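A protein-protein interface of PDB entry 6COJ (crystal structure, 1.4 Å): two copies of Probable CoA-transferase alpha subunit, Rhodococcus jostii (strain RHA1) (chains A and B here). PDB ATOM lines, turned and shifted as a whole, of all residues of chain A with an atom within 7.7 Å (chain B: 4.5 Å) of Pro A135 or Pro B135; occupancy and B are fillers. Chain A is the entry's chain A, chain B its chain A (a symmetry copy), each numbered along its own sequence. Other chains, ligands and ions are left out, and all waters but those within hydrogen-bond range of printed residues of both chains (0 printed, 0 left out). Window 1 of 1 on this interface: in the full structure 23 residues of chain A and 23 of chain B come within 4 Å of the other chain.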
ATOM      1  N   CYS A 122      16.385  22.224  23.926  1.00  0.00           N
ATOM      2  CA  CYS A 122      15.890  22.592  22.608  1.00  0.00           C
ATOM      3  C   CYS A 122      15.247  21.401  21.901  1.00  0.00           C
ATOM      4  O   CYS A 122      14.139  21.511  21.355  1.00  0.00           O
ATOM      5  CB  CYS A 122      17.065  23.144  21.807  1.00  0.00           C
ATOM      6  SG  CYS A 122      16.690  23.685  20.147  1.00  0.00           S
ATOM      7  N   ALA A 126      11.359  20.926  20.738  1.00  0.00           N
ATOM      8  CA  ALA A 126      10.924  20.637  19.375  1.00  0.00           C
ATOM      9  C   ALA A 126       9.946  19.467  19.358  1.00  0.00           C
ATOM     10  O   ALA A 126       8.878  19.540  18.737  1.00  0.00           O
ATOM     11  CB  ALA A 126      12.129  20.374  18.468  1.00  0.00           C
ATOM     12  N   ALA A 129       6.470  20.351  20.683  1.00  0.00           N
ATOM     13  CA  ALA A 129       5.698  21.105  19.703  1.00  0.00           C
ATOM     14  C   ALA A 129       5.462  20.342  18.403  1.00  0.00           C
ATOM     15  O   ALA A 129       4.907  20.915  17.459  1.00  0.00           O
ATOM     16  CB  ALA A 129       6.382  22.444  19.413  1.00  0.00           C
ATOM     17  N   LEU A 131       7.523  19.608  16.209  1.00  0.00           N
ATOM     18  CA  LEU A 131       8.322  20.192  15.146  1.00  0.00           C
ATOM     19  C   LEU A 131       9.522  19.307  14.836  1.00  0.00           C
ATOM     20  O   LEU A 131      10.043  18.626  15.722  1.00  0.00           O
ATOM     21  CB  LEU A 131       8.836  21.572  15.562  1.00  0.00           C
ATOM     22  CG  LEU A 131       7.746  22.625  15.750  1.00  0.00           C
ATOM     23  CD1 LEU A 131       8.307  23.867  16.410  1.00  0.00           C
ATOM     24  CD2 LEU A 131       7.120  22.982  14.409  1.00  0.00           C
ATOM     25  N   PRO A 132       9.989  19.285  13.589  1.00  0.00           N
ATOM     26  CA  PRO A 132      11.133  18.417  13.249  1.00  0.00           C
ATOM     27  C   PRO A 132      12.468  18.945  13.732  1.00  0.00           C
ATOM     28  O   PRO A 132      13.420  18.161  13.860  1.00  0.00           O
ATOM     29  CB  PRO A 132      11.090  18.357  11.713  1.00  0.00           C
ATOM     30  CG  PRO A 132      10.355  19.628  11.312  1.00  0.00           C
ATOM     31  CD  PRO A 132       9.364  19.901  12.406  1.00  0.00           C
ATOM     32  N   PHE A 133      12.576  20.244  13.994  1.00  0.00           N
ATOM     33  CA  PHE A 133      13.808  20.836  14.480  1.00  0.00           C
ATOM     34  C   PHE A 133      13.474  22.176  15.111  1.00  0.00           C
ATOM     35  O   PHE A 133      12.400  22.748  14.881  1.00  0.00           O
ATOM     36  CB  PHE A 133      14.805  21.068  13.339  1.00  0.00           C
ATOM     37  CG  PHE A 133      14.430  22.237  12.452  1.00  0.00           C
ATOM     38  CD1 PHE A 133      13.487  22.089  11.446  1.00  0.00           C
ATOM     39  CD2 PHE A 133      14.998  23.489  12.653  1.00  0.00           C
ATOM     40  CE1 PHE A 133      13.112  23.163  10.656  1.00  0.00           C
ATOM     41  CE2 PHE A 133      14.629  24.566  11.865  1.00  0.00           C
ATOM     42  CZ  PHE A 133      13.688  24.406  10.864  1.00  0.00           C
ATOM     43  N   LEU A 134      14.428  22.686  15.882  1.00  0.00           N
ATOM     44  CA  LEU A 134      14.468  24.096  16.251  1.00  0.00           C
ATOM     45  C   LEU A 134      15.892  24.587  16.041  1.00  0.00           C
ATOM     46  O   LEU A 134      16.847  23.835  16.282  1.00  0.00           O
ATOM     47  CB  LEU A 134      14.065  24.322  17.722  1.00  0.00           C
ATOM     48  CG  LEU A 134      12.575  24.194  18.051  1.00  0.00           C
ATOM     49  CD1 LEU A 134      12.341  24.165  19.557  1.00  0.00           C
ATOM     50  CD2 LEU A 134      11.792  25.351  17.401  1.00  0.00           C
ATOM     51  N   PRO A 135      16.070  25.817  15.575  1.00  0.00           N
ATOM     52  CA  PRO A 135      17.419  26.341  15.359  1.00  0.00           C
ATOM     53  C   PRO A 135      18.024  26.760  16.683  1.00  0.00           C
ATOM     54  O   PRO A 135      17.326  27.202  17.600  1.00  0.00           O
ATOM     55  CB  PRO A 135      17.177  27.580  14.493  1.00  0.00           C
ATOM     56  CG  PRO A 135      15.791  28.047  14.931  1.00  0.00           C
ATOM     57  CD  PRO A 135      15.024  26.784  15.186  1.00  0.00           C
ATOM     58  N   ILE A 136      19.347  26.645  16.767  1.00  0.00           N
ATOM     59  CA  ILE A 136      20.065  27.016  17.979  1.00  0.00           C
ATOM     60  C   ILE A 136      21.504  27.320  17.598  1.00  0.00           C
ATOM     61  O   ILE A 136      22.039  26.756  16.639  1.00  0.00           O
ATOM     62  CB  ILE A 136      19.951  25.906  19.058  1.00  0.00           C
ATOM     63  CG1 ILE A 136      20.513  26.368  20.408  1.00  0.00           C
ATOM     64  CG2 ILE A 136      20.675  24.638  18.618  1.00  0.00           C
ATOM     65  CD1 ILE A 136      20.089  25.498  21.614  1.00  0.00           C
ATOM     66  N   ARG A 137      22.119  28.249  18.329  1.00  0.00           N
ATOM     67  CA  ARG A 137      23.514  28.588  18.083  1.00  0.00           C
ATOM     68  C   ARG A 137      24.447  27.545  18.691  1.00  0.00           C
ATOM     69  O   ARG A 137      25.442  27.155  18.064  1.00  0.00           O
ATOM     70  CB  ARG A 137      23.814  29.967  18.666  1.00  0.00           C
ATOM     71  CG  ARG A 137      25.115  30.566  18.196  1.00  0.00           C
ATOM     72  CD  ARG A 137      25.282  32.010  18.653  1.00  0.00           C
ATOM     73  NE  ARG A 137      23.994  32.651  18.849  1.00  0.00           N
ATOM     74  CZ  ARG A 137      23.445  33.454  17.955  1.00  0.00           C
ATOM     75  NH1 ARG A 137      22.255  34.009  18.192  1.00  0.00           N
ATOM     76  NH2 ARG A 137      24.081  33.676  16.811  1.00  0.00           N
ATOM     77  N   ALA A 138      24.135  27.083  19.906  1.00  0.00           N
ATOM     78  CA  ALA A 138      24.989  26.130  20.612  1.00  0.00           C
ATOM     79  C   ALA A 138      25.276  24.909  19.752  1.00  0.00           C
ATOM     80  O   ALA A 138      24.366  24.328  19.151  1.00  0.00           O
ATOM     81  CB  ALA A 138      24.293  25.690  21.906  1.00  0.00           C
ATOM     82  N   VAL A 155      20.679  24.756   9.461  1.00  0.00           N
ATOM     83  CA  VAL A 155      19.570  25.393   8.765  1.00  0.00           C
ATOM     84  C   VAL A 155      19.925  26.860   8.591  1.00  0.00           C
ATOM     85  O   VAL A 155      20.448  27.495   9.513  1.00  0.00           O
ATOM     86  CB  VAL A 155      18.237  25.210   9.529  1.00  0.00           C
ATOM     87  CG1 VAL A 155      18.328  25.794  10.938  1.00  0.00           C
ATOM     88  CG2 VAL A 155      17.079  25.834   8.754  1.00  0.00           C
ATOM     89  N   THR A 156      19.673  27.394   7.401  1.00  0.00           N
ATOM     90  CA  THR A 156      19.961  28.792   7.106  1.00  0.00           C
ATOM     91  C   THR A 156      18.701  29.643   7.216  1.00  0.00           C
ATOM     92  O   THR A 156      17.630  29.254   6.742  1.00  0.00           O
ATOM     93  CB  THR A 156      20.569  28.907   5.713  1.00  0.00           C
ATOM     94  OG1 THR A 156      21.800  28.181   5.695  1.00  0.00           O
ATOM     95  CG2 THR A 156      20.857  30.360   5.361  1.00  0.00           C
ATOM     96  N   SER A 157      18.832  30.794   7.862  1.00  0.00           N
ATOM     97  CA  SER A 157      17.715  31.718   7.980  1.00  0.00           C
ATOM     98  C   SER A 157      17.247  32.175   6.604  1.00  0.00           C
ATOM     99  O   SER A 157      18.076  32.581   5.780  1.00  0.00           O
ATOM    100  CB  SER A 157      18.141  32.948   8.763  1.00  0.00           C
ATOM    101  OG  SER A 157      17.069  33.871   8.832  1.00  0.00           O
ATOM    102  N   THR A 168      23.544  30.827   9.489  1.00  0.00           N
ATOM    103  CA  THR A 168      23.371  29.382   9.430  1.00  0.00           C
ATOM    104  C   THR A 168      23.558  28.837  10.841  1.00  0.00           C
ATOM    105  O   THR A 168      24.593  29.076  11.471  1.00  0.00           O
ATOM    106  CB  THR A 168      24.365  28.753   8.457  1.00  0.00           C
ATOM    107  OG1 THR A 168      24.098  29.240   7.137  1.00  0.00           O
ATOM    108  CG2 THR A 168      24.218  27.253   8.441  1.00  0.00           C
ATOM    109  N   LEU A 169      22.540  28.152  11.343  1.00  0.00           N
ATOM    110  CA  LEU A 169      22.479  27.712  12.729  1.00  0.00           C
ATOM    111  C   LEU A 169      22.370  26.192  12.785  1.00  0.00           C
ATOM    112  O   LEU A 169      22.085  25.530  11.786  1.00  0.00           O
ATOM    113  CB  LEU A 169      21.268  28.347  13.420  1.00  0.00           C
ATOM    114  CG  LEU A 169      21.299  29.873  13.483  1.00  0.00           C
ATOM    115  CD1 LEU A 169      19.885  30.444  13.483  1.00  0.00           C
ATOM    116  CD2 LEU A 169      22.076  30.298  14.705  1.00  0.00           C
ATOM    117  N   ILE A 170      22.610  25.626  13.967  1.00  0.00           N
ATOM    118  CA  ILE A 170      22.335  24.206  14.166  1.00  0.00           C
ATOM    119  C   ILE A 170      20.834  23.988  14.059  1.00  0.00           C
ATOM    120  O   ILE A 170      20.044  24.721  14.666  1.00  0.00           O
ATOM    121  CB  ILE A 170      22.833  23.751  15.546  1.00  0.00           C
ATOM    122  CG1 ILE A 170      24.340  23.984  15.703  1.00  0.00           C
ATOM    123  CG2 ILE A 170      22.455  22.297  15.803  1.00  0.00           C
ATOM    124  CD1 ILE A 170      25.209  23.130  14.785  1.00  0.00           C
ATOM    125  N   ALA A 171      20.424  22.989  13.288  1.00  0.00           N
ATOM    126  CA  ALA A 171      19.035  22.532  13.310  1.00  0.00           C
ATOM    127  C   ALA A 171      18.974  21.399  14.321  1.00  0.00           C
ATOM    128  O   ALA A 171      19.295  20.249  14.005  1.00  0.00           O
ATOM    129  CB  ALA A 171      18.606  22.058  11.924  1.00  0.00           C
ATOM    130  N   MET A 172      18.621  21.709  15.558  1.00  0.00           N
ATOM    131  CA  MET A 172      18.529  20.651  16.552  1.00  0.00           C
ATOM    132  C   MET A 172      17.324  19.779  16.236  1.00  0.00           C
ATOM    133  O   MET A 172      16.194  20.277  16.246  1.00  0.00           O
ATOM    134  CB  MET A 172      18.376  21.264  17.939  1.00  0.00           C
ATOM    135  CG  MET A 172      18.214  20.210  19.021  1.00  0.00           C
ATOM    136  SD  MET A 172      19.680  19.177  19.167  1.00  0.00           S
ATOM    137  CE  MET A 172      18.962  17.833  20.096  1.00  0.00           C
ATOM    138  N   PRO A 173      17.503  18.494  15.938  1.00  0.00           N
ATOM    139  CA  PRO A 173      16.342  17.648  15.652  1.00  0.00           C
ATOM    140  C   PRO A 173      15.524  17.402  16.912  1.00  0.00           C
ATOM    141  O   PRO A 173      16.033  17.428  18.039  1.00  0.00           O
ATOM    142  CB  PRO A 173      16.976  16.342  15.158  1.00  0.00           C
ATOM    143  CG  PRO A 173      18.289  16.291  15.905  1.00  0.00           C
ATOM    144  CD  PRO A 173      18.763  17.729  15.915  1.00  0.00           C
ATOM    145  N   CYS B 122       6.074  33.378  19.624  1.00  0.00           N
ATOM    146  CA  CYS B 122       7.197  32.804  18.900  1.00  0.00           C
ATOM    147  C   CYS B 122       8.191  33.879  18.466  1.00  0.00           C
ATOM    148  O   CYS B 122       9.406  33.733  18.661  1.00  0.00           O
ATOM    149  CB  CYS B 122       6.638  32.049  17.697  1.00  0.00           C
ATOM    150  SG  CYS B 122       7.843  31.235  16.660  1.00  0.00           S
ATOM    151  N   LEU B 131      17.862  35.031  17.828  1.00  0.00           N
ATOM    152  CA  LEU B 131      17.759  34.218  16.629  1.00  0.00           C
ATOM    153  C   LEU B 131      16.987  34.962  15.548  1.00  0.00           C
ATOM    154  O   LEU B 131      16.100  35.763  15.850  1.00  0.00           O
ATOM    155  CB  LEU B 131      17.024  32.911  16.933  1.00  0.00           C
ATOM    156  CG  LEU B 131      17.763  31.974  17.885  1.00  0.00           C
ATOM    157  CD1 LEU B 131      16.860  30.844  18.335  1.00  0.00           C
ATOM    158  CD2 LEU B 131      19.008  31.412  17.213  1.00  0.00           C
ATOM    159  N   PHE B 133      14.873  33.716  13.336  1.00  0.00           N
ATOM    160  CA  PHE B 133      13.548  33.155  13.153  1.00  0.00           C
ATOM    161  C   PHE B 133      13.398  31.974  14.095  1.00  0.00           C
ATOM    162  O   PHE B 133      14.383  31.431  14.612  1.00  0.00           O
ATOM    163  CB  PHE B 133      13.344  32.661  11.715  1.00  0.00           C
ATOM    164  CG  PHE B 133      14.083  31.372  11.420  1.00  0.00           C
ATOM    165  CD1 PHE B 133      15.433  31.386  11.104  1.00  0.00           C
ATOM    166  CD2 PHE B 133      13.429  30.148  11.496  1.00  0.00           C
ATOM    167  CE1 PHE B 133      16.123  30.209  10.869  1.00  0.00           C
ATOM    168  CE2 PHE B 133      14.113  28.969  11.261  1.00  0.00           C
ATOM    169  CZ  PHE B 133      15.460  28.995  10.945  1.00  0.00           C
ATOM    170  N   LEU B 134      12.149  31.561  14.282  1.00  0.00           N
ATOM    171  CA  LEU B 134      11.831  30.243  14.817  1.00  0.00           C
ATOM    172  C   LEU B 134      10.740  29.642  13.944  1.00  0.00           C
ATOM    173  O   LEU B 134       9.857  30.370  13.469  1.00  0.00           O
ATOM    174  CB  LEU B 134      11.333  30.313  16.275  1.00  0.00           C
ATOM    175  CG  LEU B 134      12.391  30.583  17.348  1.00  0.00           C
ATOM    176  CD1 LEU B 134      11.748  30.901  18.693  1.00  0.00           C
ATOM    177  CD2 LEU B 134      13.336  29.372  17.469  1.00  0.00           C
ATOM    178  N   PRO B 135      10.782  28.339  13.693  1.00  0.00           N
ATOM    179  CA  PRO B 135       9.755  27.709  12.863  1.00  0.00           C
ATOM    180  C   PRO B 135       8.493  27.506  13.675  1.00  0.00           C
ATOM    181  O   PRO B 135       8.536  27.280  14.887  1.00  0.00           O
ATOM    182  CB  PRO B 135      10.369  26.348  12.523  1.00  0.00           C
ATOM    183  CG  PRO B 135      11.247  26.048  13.735  1.00  0.00           C
ATOM    184  CD  PRO B 135      11.811  27.378  14.138  1.00  0.00           C
ATOM    185  N   ILE B 136       7.357  27.560  12.985  1.00  0.00           N
ATOM    186  CA  ILE B 136       6.065  27.378  13.635  1.00  0.00           C
ATOM    187  C   ILE B 136       5.069  26.929  12.581  1.00  0.00           C
ATOM    188  O   ILE B 136       5.190  27.276  11.403  1.00  0.00           O
ATOM    189  CB  ILE B 136       5.622  28.672  14.369  1.00  0.00           C
ATOM    190  CG1 ILE B 136       4.379  28.433  15.234  1.00  0.00           C
ATOM    191  CG2 ILE B 136       5.338  29.794  13.377  1.00  0.00           C
ATOM    192  CD1 ILE B 136       4.107  29.533  16.288  1.00  0.00           C
ATOM    193  N   VAL B 155      10.428  28.000   5.978  1.00  0.00           N
ATOM    194  CA  VAL B 155      11.699  27.310   6.149  1.00  0.00           C
ATOM    195  C   VAL B 155      11.419  25.818   6.079  1.00  0.00           C
ATOM    196  O   VAL B 155      10.437  25.334   6.652  1.00  0.00           O
ATOM    197  CB  VAL B 155      12.388  27.704   7.477  1.00  0.00           C
ATOM    198  CG1 VAL B 155      11.496  27.384   8.675  1.00  0.00           C
ATOM    199  CG2 VAL B 155      13.745  27.015   7.609  1.00  0.00           C
ATOM    200  N   LEU B 169       7.647  24.907   7.089  1.00  0.00           N
ATOM    201  CA  LEU B 169       6.950  25.597   8.166  1.00  0.00           C
ATOM    202  C   LEU B 169       7.094  27.104   7.993  1.00  0.00           C
ATOM    203  O   LEU B 169       7.925  27.587   7.221  1.00  0.00           O
ATOM    204  CB  LEU B 169       7.532  25.168   9.516  1.00  0.00           C
ATOM    205  CG  LEU B 169       7.386  23.680   9.829  1.00  0.00           C
ATOM    206  CD1 LEU B 169       8.525  23.199  10.721  1.00  0.00           C
ATOM    207  CD2 LEU B 169       6.037  23.443  10.464  1.00  0.00           C
ATOM    208  N   ILE B 170       6.270  27.863   8.712  1.00  0.00           N
ATOM    209  CA  ILE B 170       6.467  29.309   8.766  1.00  0.00           C
ATOM    210  C   ILE B 170       7.782  29.587   9.476  1.00  0.00           C
ATOM    211  O   ILE B 170       8.057  29.024  10.542  1.00  0.00           O
ATOM    212  CB  ILE B 170       5.311  29.980   9.524  1.00  0.00           C
ATOM    213  CG1 ILE B 170       3.962  29.695   8.855  1.00  0.00           C
ATOM    214  CG2 ILE B 170       5.563  31.475   9.676  1.00  0.00           C
ATOM    215  CD1 ILE B 170       3.801  30.316   7.470  1.00  0.00           C
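Leu A131 touches Leu B169, and with the chains exchanged Leu A169 touches Leu B131.
Phe A133 touches Pro B135, and with the chains exchanged Pro A135 touches Phe B133.
Leu A134 touches Pro B135, and with the chains exchanged Pro A135 touches Leu B134.
Pro A135 touches its own counterpart, Pro B135.
Positions printed for both chains: 122, 131, 133, 134, 135, 136, 155, 169 and 170.
Of the 12 pairs that touch across the chains among the printed residues, 10 have their exchanged pair printed and touching as well.
Of the 9 printed residues of chain B, 6 touch a printed residue of chain A.
Of the 20 printed residues of chain A, 8 touch a printed residue of chain B.
Hydrophobic or aromatic side chains of chain A that line the printed part of chain B: Leu A131, Pro A132, Leu A134, Pro A135, Val A155 and Leu A169.
Among the printed residues, no Asp or Glu carboxylate lies within 4 Å of a Lys or Arg side-chain nitrogen of the other chain.
O of Ala A126 lies within hydrogen-bond range of N of Leu A131, 2.9 Å away.
N of Met A172 sits at hydrogen-bond distance from O of Leu A134 (2.9 Å).
The backbone NH of Val A155 lies within hydrogen-bond range of the backbone carbonyl oxygen of Leu A169, at 2.8 Å.
O of Leu B169 is in hydrogen-bond range of N of Val B155 (2.8 Å).
Pro A135 touches just these residues of chain B: Leu B131 (3.7 Å), Phe B133 (3.7 Å), Leu B134 (3.8 Å) and Pro B135 (3.4 Å).
Of the printed residues of chain A, Val B155 touches Val A155 (3.7 Å).
Of the printed residues of chain B, Leu A131 touches Pro B135 and Leu B169.
Met A172 touches none of the printed residues of chain B.
O of Pro B135 touches CD1 of Leu A131, 3.7 Å away.
Leu A131 touches Leu B169 (CD2 to CD1, 3.95 Å).
Pro A132 touches Leu B169 (CD to CD1, 3.8 Å).
Pro B135 touches Phe A133 (CG to O, 3.7 Å).
CG of Pro B135 touches CD2 of Leu A134, at 3.8 Å.
CG of Pro A135 touches O of Phe B133 (3.7 Å).
Pro A135 touches Pro B135 (CD to CD, 3.4 Å).
Val B155 touches Val A155.
Ser A157 touches Phe B133.
Leu B131 touches Leu A169.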
